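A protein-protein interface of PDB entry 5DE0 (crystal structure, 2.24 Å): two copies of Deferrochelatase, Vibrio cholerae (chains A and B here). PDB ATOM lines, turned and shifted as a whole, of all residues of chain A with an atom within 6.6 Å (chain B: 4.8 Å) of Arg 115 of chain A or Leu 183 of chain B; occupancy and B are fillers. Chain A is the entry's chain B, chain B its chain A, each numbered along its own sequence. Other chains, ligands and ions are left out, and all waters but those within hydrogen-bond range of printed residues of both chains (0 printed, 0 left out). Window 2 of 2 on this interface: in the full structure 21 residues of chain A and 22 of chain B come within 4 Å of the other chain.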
ATOM      1  N   LEU A 110     -12.108  -1.905 -15.878  1.00  0.00           N
ATOM      2  CA  LEU A 110     -12.054  -0.819 -14.905  1.00  0.00           C
ATOM      3  C   LEU A 110     -11.475  -1.321 -13.590  1.00  0.00           C
ATOM      4  O   LEU A 110     -10.592  -0.693 -13.006  1.00  0.00           O
ATOM      5  CB  LEU A 110     -13.445  -0.224 -14.672  1.00  0.00           C
ATOM      6  CG  LEU A 110     -14.175   0.342 -15.892  1.00  0.00           C
ATOM      7  CD1 LEU A 110     -15.568   0.802 -15.495  1.00  0.00           C
ATOM      8  CD2 LEU A 110     -13.388   1.481 -16.520  1.00  0.00           C
ATOM      9  N   PHE A 111     -11.984  -2.458 -13.129  1.00  0.00           N
ATOM     10  CA  PHE A 111     -11.464  -3.102 -11.931  1.00  0.00           C
ATOM     11  C   PHE A 111      -9.997  -3.468 -12.124  1.00  0.00           C
ATOM     12  O   PHE A 111      -9.178  -3.272 -11.225  1.00  0.00           O
ATOM     13  CB  PHE A 111     -12.285  -4.349 -11.586  1.00  0.00           C
ATOM     14  CG  PHE A 111     -11.822  -5.060 -10.342  1.00  0.00           C
ATOM     15  CD1 PHE A 111     -10.815  -6.013 -10.402  1.00  0.00           C
ATOM     16  CD2 PHE A 111     -12.397  -4.778  -9.114  1.00  0.00           C
ATOM     17  CE1 PHE A 111     -10.387  -6.662  -9.264  1.00  0.00           C
ATOM     18  CE2 PHE A 111     -11.976  -5.428  -7.971  1.00  0.00           C
ATOM     19  CZ  PHE A 111     -10.969  -6.371  -8.045  1.00  0.00           C
ATOM     20  N   TYR A 112      -9.671  -4.002 -13.299  1.00  0.00           N
ATOM     21  CA  TYR A 112      -8.302  -4.421 -13.589  1.00  0.00           C
ATOM     22  C   TYR A 112      -7.341  -3.239 -13.598  1.00  0.00           C
ATOM     23  O   TYR A 112      -6.220  -3.342 -13.105  1.00  0.00           O
ATOM     24  CB  TYR A 112      -8.226  -5.158 -14.930  1.00  0.00           C
ATOM     25  CG  TYR A 112      -6.810  -5.472 -15.369  1.00  0.00           C
ATOM     26  CD1 TYR A 112      -6.127  -6.564 -14.848  1.00  0.00           C
ATOM     27  CD2 TYR A 112      -6.155  -4.672 -16.301  1.00  0.00           C
ATOM     28  CE1 TYR A 112      -4.832  -6.853 -15.243  1.00  0.00           C
ATOM     29  CE2 TYR A 112      -4.862  -4.953 -16.700  1.00  0.00           C
ATOM     30  CZ  TYR A 112      -4.204  -6.043 -16.169  1.00  0.00           C
ATOM     31  OH  TYR A 112      -2.916  -6.324 -16.566  1.00  0.00           O
ATOM     32  N   THR A 113      -7.781  -2.122 -14.169  1.00  0.00           N
ATOM     33  CA  THR A 113      -6.937  -0.935 -14.268  1.00  0.00           C
ATOM     34  C   THR A 113      -6.578  -0.401 -12.886  1.00  0.00           C
ATOM     35  O   THR A 113      -5.444   0.014 -12.645  1.00  0.00           O
ATOM     36  CB  THR A 113      -7.623   0.179 -15.082  1.00  0.00           C
ATOM     37  OG1 THR A 113      -7.898  -0.298 -16.405  1.00  0.00           O
ATOM     38  CG2 THR A 113      -6.733   1.411 -15.169  1.00  0.00           C
ATOM     39  N   LEU A 114      -7.544  -0.433 -11.975  1.00  0.00           N
ATOM     40  CA  LEU A 114      -7.318   0.052 -10.620  1.00  0.00           C
ATOM     41  C   LEU A 114      -6.451  -0.914  -9.819  1.00  0.00           C
ATOM     42  O   LEU A 114      -5.514  -0.491  -9.145  1.00  0.00           O
ATOM     43  CB  LEU A 114      -8.648   0.284  -9.900  1.00  0.00           C
ATOM     44  CG  LEU A 114      -8.526   0.830  -8.476  1.00  0.00           C
ATOM     45  CD1 LEU A 114      -7.726   2.124  -8.467  1.00  0.00           C
ATOM     46  CD2 LEU A 114      -9.900   1.041  -7.862  1.00  0.00           C
ATOM     47  N   ARG A 115      -6.762  -2.206  -9.895  1.00  0.00           N
ATOM     48  CA  ARG A 115      -6.005  -3.215  -9.154  1.00  0.00           C
ATOM     49  C   ARG A 115      -4.550  -3.265  -9.610  1.00  0.00           C
ATOM     50  O   ARG A 115      -3.634  -3.224  -8.792  1.00  0.00           O
ATOM     51  CB  ARG A 115      -6.643  -4.599  -9.305  1.00  0.00           C
ATOM     52  CG  ARG A 115      -5.942  -5.681  -8.487  1.00  0.00           C
ATOM     53  CD  ARG A 115      -6.582  -7.052  -8.661  1.00  0.00           C
ATOM     54  NE  ARG A 115      -6.354  -7.611  -9.991  1.00  0.00           N
ATOM     55  CZ  ARG A 115      -6.684  -8.850 -10.349  1.00  0.00           C
ATOM     56  NH1 ARG A 115      -7.255  -9.666  -9.473  1.00  0.00           N
ATOM     57  NH2 ARG A 115      -6.439  -9.274 -11.582  1.00  0.00           N
ATOM     58  N   LYS A 116      -4.350  -3.352 -10.920  1.00  0.00           N
ATOM     59  CA  LYS A 116      -3.011  -3.409 -11.496  1.00  0.00           C
ATOM     60  C   LYS A 116      -2.279  -2.078 -11.343  1.00  0.00           C
ATOM     61  O   LYS A 116      -1.066  -2.045 -11.135  1.00  0.00           O
ATOM     62  CB  LYS A 116      -3.089  -3.798 -12.976  1.00  0.00           C
ATOM     63  CG  LYS A 116      -1.752  -3.873 -13.689  1.00  0.00           C
ATOM     64  CD  LYS A 116      -0.912  -5.022 -13.165  1.00  0.00           C
ATOM     65  CE  LYS A 116       0.362  -5.182 -13.978  1.00  0.00           C
ATOM     66  NZ  LYS A 116       1.184  -6.327 -13.493  1.00  0.00           N
ATOM     67  N   GLY A 117      -3.026  -0.983 -11.443  1.00  0.00           N
ATOM     68  CA  GLY A 117      -2.446   0.347 -11.403  1.00  0.00           C
ATOM     69  C   GLY A 117      -1.872   0.764 -10.061  1.00  0.00           C
ATOM     70  O   GLY A 117      -0.924   1.544 -10.005  1.00  0.00           O
ATOM     71  N   ILE A 118      -2.445   0.251  -8.976  1.00  0.00           N
ATOM     72  CA  ILE A 118      -2.010   0.640  -7.636  1.00  0.00           C
ATOM     73  C   ILE A 118      -1.392  -0.528  -6.874  1.00  0.00           C
ATOM     74  O   ILE A 118      -1.167  -0.438  -5.667  1.00  0.00           O
ATOM     75  CB  ILE A 118      -3.177   1.211  -6.800  1.00  0.00           C
ATOM     76  CG1 ILE A 118      -4.145   0.100  -6.389  1.00  0.00           C
ATOM     77  CG2 ILE A 118      -3.894   2.315  -7.562  1.00  0.00           C
ATOM     78  CD1 ILE A 118      -5.247   0.555  -5.463  1.00  0.00           C
ATOM     79  N   SER A 119      -1.116  -1.616  -7.588  1.00  0.00           N
ATOM     80  CA  SER A 119      -0.621  -2.847  -6.978  1.00  0.00           C
ATOM     81  C   SER A 119       0.638  -2.635  -6.137  1.00  0.00           C
ATOM     82  O   SER A 119       0.776  -3.217  -5.063  1.00  0.00           O
ATOM     83  CB  SER A 119      -0.349  -3.897  -8.058  1.00  0.00           C
ATOM     84  OG  SER A 119       0.027  -5.135  -7.480  1.00  0.00           O
ATOM     85  N   ASP A 120       1.546  -1.792  -6.622  1.00  0.00           N
ATOM     86  CA  ASP A 120       2.811  -1.553  -5.934  1.00  0.00           C
ATOM     87  C   ASP A 120       2.705  -0.508  -4.822  1.00  0.00           C
ATOM     88  O   ASP A 120       3.573  -0.430  -3.952  1.00  0.00           O
ATOM     89  CB  ASP A 120       3.886  -1.122  -6.934  1.00  0.00           C
ATOM     90  CG  ASP A 120       4.285  -2.237  -7.882  1.00  0.00           C
ATOM     91  OD1 ASP A 120       4.054  -3.419  -7.547  1.00  0.00           O
ATOM     92  OD2 ASP A 120       4.837  -1.931  -8.960  1.00  0.00           O
ATOM     93  N   TYR A 132     -18.190   2.367  -8.832  1.00  0.00           N
ATOM     94  CA  TYR A 132     -18.336   1.856 -10.188  1.00  0.00           C
ATOM     95  C   TYR A 132     -19.683   2.267 -10.766  1.00  0.00           C
ATOM     96  O   TYR A 132     -20.729   1.770 -10.342  1.00  0.00           O
ATOM     97  CB  TYR A 132     -18.189   0.335 -10.210  1.00  0.00           C
ATOM     98  CG  TYR A 132     -16.785  -0.147  -9.916  1.00  0.00           C
ATOM     99  CD1 TYR A 132     -16.375  -0.402  -8.613  1.00  0.00           C
ATOM    100  CD2 TYR A 132     -15.869  -0.345 -10.942  1.00  0.00           C
ATOM    101  CE1 TYR A 132     -15.095  -0.840  -8.339  1.00  0.00           C
ATOM    102  CE2 TYR A 132     -14.585  -0.784 -10.676  1.00  0.00           C
ATOM    103  CZ  TYR A 132     -14.204  -1.030  -9.373  1.00  0.00           C
ATOM    104  OH  TYR A 132     -12.928  -1.466  -9.103  1.00  0.00           O
ATOM    105  N   TYR B 136     -14.656 -11.629 -15.755  1.00  0.00           N
ATOM    106  CA  TYR B 136     -13.434 -10.850 -15.600  1.00  0.00           C
ATOM    107  C   TYR B 136     -12.359 -11.290 -16.588  1.00  0.00           C
ATOM    108  O   TYR B 136     -11.862 -12.415 -16.513  1.00  0.00           O
ATOM    109  CB  TYR B 136     -12.927 -10.972 -14.161  1.00  0.00           C
ATOM    110  CG  TYR B 136     -11.714 -10.135 -13.841  1.00  0.00           C
ATOM    111  CD1 TYR B 136     -11.794  -8.749 -13.782  1.00  0.00           C
ATOM    112  CD2 TYR B 136     -10.492 -10.733 -13.572  1.00  0.00           C
ATOM    113  CE1 TYR B 136     -10.684  -7.982 -13.479  1.00  0.00           C
ATOM    114  CE2 TYR B 136      -9.377  -9.976 -13.266  1.00  0.00           C
ATOM    115  CZ  TYR B 136      -9.478  -8.602 -13.222  1.00  0.00           C
ATOM    116  OH  TYR B 136      -8.367  -7.850 -12.918  1.00  0.00           O
ATOM    117  N   MET B 142     -10.265 -13.675 -10.012  1.00  0.00           N
ATOM    118  CA  MET B 142      -9.358 -12.589  -9.643  1.00  0.00           C
ATOM    119  C   MET B 142      -8.016 -13.088  -9.110  1.00  0.00           C
ATOM    120  O   MET B 142      -7.118 -12.293  -8.837  1.00  0.00           O
ATOM    121  CB  MET B 142     -10.028 -11.674  -8.617  1.00  0.00           C
ATOM    122  CG  MET B 142     -11.149 -10.837  -9.207  1.00  0.00           C
ATOM    123  SD  MET B 142     -12.084  -9.910  -7.984  1.00  0.00           S
ATOM    124  CE  MET B 142     -13.224  -9.023  -9.040  1.00  0.00           C
ATOM    125  N   THR B 143      -7.880 -14.404  -8.975  1.00  0.00           N
ATOM    126  CA  THR B 143      -6.596 -15.009  -8.636  1.00  0.00           C
ATOM    127  C   THR B 143      -5.697 -15.087  -9.867  1.00  0.00           C
ATOM    128  O   THR B 143      -4.502 -15.359  -9.761  1.00  0.00           O
ATOM    129  CB  THR B 143      -6.767 -16.424  -8.048  1.00  0.00           C
ATOM    130  OG1 THR B 143      -7.580 -17.214  -8.925  1.00  0.00           O
ATOM    131  CG2 THR B 143      -7.420 -16.359  -6.673  1.00  0.00           C
ATOM    132  N   HIS B 181     -11.247 -12.922  -1.173  1.00  0.00           N
ATOM    133  CA  HIS B 181      -9.864 -13.248  -1.515  1.00  0.00           C
ATOM    134  C   HIS B 181      -8.837 -12.418  -0.755  1.00  0.00           C
ATOM    135  O   HIS B 181      -9.035 -11.228  -0.510  1.00  0.00           O
ATOM    136  CB  HIS B 181      -9.626 -13.064  -3.017  1.00  0.00           C
ATOM    137  CG  HIS B 181     -10.322 -14.077  -3.872  1.00  0.00           C
ATOM    138  ND1 HIS B 181     -11.244 -14.970  -3.371  1.00  0.00           N
ATOM    139  CD2 HIS B 181     -10.227 -14.336  -5.197  1.00  0.00           C
ATOM    140  CE1 HIS B 181     -11.689 -15.736  -4.352  1.00  0.00           C
ATOM    141  NE2 HIS B 181     -11.088 -15.371  -5.470  1.00  0.00           N
ATOM    142  N   ASN B 182      -7.732 -13.062  -0.396  1.00  0.00           N
ATOM    143  CA  ASN B 182      -6.572 -12.376   0.157  1.00  0.00           C
ATOM    144  C   ASN B 182      -5.485 -12.299  -0.910  1.00  0.00           C
ATOM    145  O   ASN B 182      -4.521 -13.061  -0.881  1.00  0.00           O
ATOM    146  CB  ASN B 182      -6.058 -13.099   1.406  1.00  0.00           C
ATOM    147  CG  ASN B 182      -5.023 -12.290   2.174  1.00  0.00           C
ATOM    148  OD1 ASN B 182      -4.272 -11.502   1.599  1.00  0.00           O
ATOM    149  ND2 ASN B 182      -4.981 -12.488   3.485  1.00  0.00           N
ATOM    150  N   LEU B 183      -5.653 -11.374  -1.851  1.00  0.00           N
ATOM    151  CA  LEU B 183      -4.769 -11.273  -3.013  1.00  0.00           C
ATOM    152  C   LEU B 183      -3.281 -11.014  -2.709  1.00  0.00           C
ATOM    153  O   LEU B 183      -2.422 -11.609  -3.362  1.00  0.00           O
ATOM    154  CB  LEU B 183      -5.289 -10.188  -3.964  1.00  0.00           C
ATOM    155  CG  LEU B 183      -6.599 -10.501  -4.689  1.00  0.00           C
ATOM    156  CD1 LEU B 183      -6.920  -9.421  -5.710  1.00  0.00           C
ATOM    157  CD2 LEU B 183      -6.542 -11.871  -5.354  1.00  0.00           C
ATOM    158  N   PRO B 184      -2.961 -10.125  -1.744  1.00  0.00           N
ATOM    159  CA  PRO B 184      -1.529  -9.925  -1.471  1.00  0.00           C
ATOM    160  C   PRO B 184      -0.812 -11.185  -0.983  1.00  0.00           C
ATOM    161  O   PRO B 184       0.337 -11.416  -1.361  1.00  0.00           O
ATOM    162  CB  PRO B 184      -1.530  -8.850  -0.379  1.00  0.00           C
ATOM    163  CG  PRO B 184      -2.794  -8.098  -0.599  1.00  0.00           C
ATOM    164  CD  PRO B 184      -3.788  -9.138  -1.021  1.00  0.00           C
ATOM    165  N   ALA B 185      -1.480 -11.983  -0.157  1.00  0.00           N
ATOM    166  CA  ALA B 185      -0.910 -13.239   0.318  1.00  0.00           C
ATOM    167  C   ALA B 185      -0.740 -14.217  -0.841  1.00  0.00           C
ATOM    168  O   ALA B 185       0.254 -14.938  -0.923  1.00  0.00           O
ATOM    169  CB  ALA B 185      -1.785 -13.844   1.405  1.00  0.00           C
ATOM    170  N   TRP B 186      -1.722 -14.226  -1.735  1.00  0.00           N
ATOM    171  CA  TRP B 186      -1.685 -15.050  -2.938  1.00  0.00           C
ATOM    172  C   TRP B 186      -0.604 -14.553  -3.893  1.00  0.00           C
ATOM    173  O   TRP B 186      -0.052 -15.320  -4.683  1.00  0.00           O
ATOM    174  CB  TRP B 186      -3.058 -15.042  -3.617  1.00  0.00           C
ATOM    175  CG  TRP B 186      -3.127 -15.729  -4.954  1.00  0.00           C
ATOM    176  CD1 TRP B 186      -3.152 -15.133  -6.182  1.00  0.00           C
ATOM    177  CD2 TRP B 186      -3.205 -17.139  -5.193  1.00  0.00           C
ATOM    178  NE1 TRP B 186      -3.233 -16.084  -7.171  1.00  0.00           N
ATOM    179  CE2 TRP B 186      -3.267 -17.325  -6.589  1.00  0.00           C
ATOM    180  CE3 TRP B 186      -3.224 -18.265  -4.363  1.00  0.00           C
ATOM    181  CZ2 TRP B 186      -3.347 -18.587  -7.172  1.00  0.00           C
ATOM    182  CZ3 TRP B 186      -3.304 -19.520  -4.945  1.00  0.00           C
ATOM    183  CH2 TRP B 186      -3.363 -19.670  -6.335  1.00  0.00           C
ATOM    184  N   ASN B 187      -0.302 -13.262  -3.801  1.00  0.00           N
ATOM    185  CA  ASN B 187       0.672 -12.621  -4.676  1.00  0.00           C
ATOM    186  C   ASN B 187       2.116 -12.943  -4.295  1.00  0.00           C
ATOM    187  O   ASN B 187       3.008 -12.917  -5.143  1.00  0.00           O
ATOM    188  CB  ASN B 187       0.460 -11.103  -4.668  1.00  0.00           C
ATOM    189  CG  ASN B 187       1.384 -10.376  -5.624  1.00  0.00           C
ATOM    190  OD1 ASN B 187       1.771 -10.911  -6.662  1.00  0.00           O
ATOM    191  ND2 ASN B 187       1.744  -9.146  -5.276  1.00  0.00           N
ATOM    192  N   VAL B 241     -11.820  -3.101  -5.271  1.00  0.00           N
ATOM    193  CA  VAL B 241     -10.421  -3.214  -4.888  1.00  0.00           C
ATOM    194  C   VAL B 241     -10.218  -2.899  -3.405  1.00  0.00           C
ATOM    195  O   VAL B 241      -9.525  -3.632  -2.697  1.00  0.00           O
ATOM    196  CB  VAL B 241      -9.537  -2.281  -5.743  1.00  0.00           C
ATOM    197  CG1 VAL B 241      -8.088  -2.346  -5.288  1.00  0.00           C
ATOM    198  CG2 VAL B 241      -9.653  -2.653  -7.214  1.00  0.00           C
ATOM    199  N   HIS B 245     -13.610  -8.529  -2.297  1.00  0.00           N
ATOM    200  CA  HIS B 245     -13.570  -8.974  -3.681  1.00  0.00           C
ATOM    201  C   HIS B 245     -13.171 -10.439  -3.738  1.00  0.00           C
ATOM    202  O   HIS B 245     -12.482 -10.941  -2.851  1.00  0.00           O
ATOM    203  CB  HIS B 245     -12.605  -8.121  -4.509  1.00  0.00           C
ATOM    204  CG  HIS B 245     -11.210  -8.074  -3.962  1.00  0.00           C
ATOM    205  ND1 HIS B 245     -10.717  -6.987  -3.276  1.00  0.00           N
ATOM    206  CD2 HIS B 245     -10.207  -8.983  -4.005  1.00  0.00           C
ATOM    207  CE1 HIS B 245      -9.466  -7.227  -2.916  1.00  0.00           C
ATOM    208  NE2 HIS B 245      -9.134  -8.428  -3.345  1.00  0.00           N
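No position is printed for both chains.
Printed residues of chain B within 4 Å of Leu 114 of chain A: Val 241 (3.8 Å).
Arg 115 of chain A touches just these residues of chain B: Tyr 136, Met 142, Leu 183 and Val 241.
Of the printed residues of chain A, Met 142 of chain B touches Phe 111 (3.6 Å) and Arg 115 (2.7 Å).
Leu 183 of chain B touches one residue of chain A.
Ala 185 of chain B touches none of the printed residues of chain A.
The nearest printed residue of chain A that does not touch Val 241 of chain B is Ile 118 of chain A (4.1 Å).
The guanidinium group of Arg 115 of chain A lies within hydrogen-bond range of the side-chain hydroxyl of Tyr 136 of chain B.
The guanidinium group of Arg 115 of chain A lies within hydrogen-bond range of the backbone carbonyl oxygen of Met 142 of chain B (2.7 Å).
Of the 12 printed residues of chain B, 4 touch a printed residue of chain A.
Printed residues of chain B that touch a printed residue of chain A: Tyr 136, Met 142, Leu 183 and Val 241.
Printed residues of chain A that touch a printed residue of chain B: Phe 111, Tyr 112, Leu 114, Arg 115 and Tyr 132.
Among the printed residues, no Asp or Glu carboxylate lies within 4 Å of a Lys or Arg side-chain nitrogen of the other chain.
Tyr 136 of chain B touches Phe 111 of chain A.
Met 142 of chain B touches Phe 111 of chain A.
CE2 of Phe 111 of chain A touches N of Val 241 of chain B (3.6 Å).
Tyr 112 of chain A touches Tyr 136 of chain B.
CD2 of Leu 114 of chain A touches CG2 of Val 241 of chain B, at 3.8 Å.
Arg 115 of chain A touches Leu 183 of chain B (NH1 to CD1, 3.8 Å).
Val 241 of chain B touches Arg 115 of chain A.
Tyr 132 of chain A touches Val 241 of chain B (OH to CG2, 3.96 Å).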
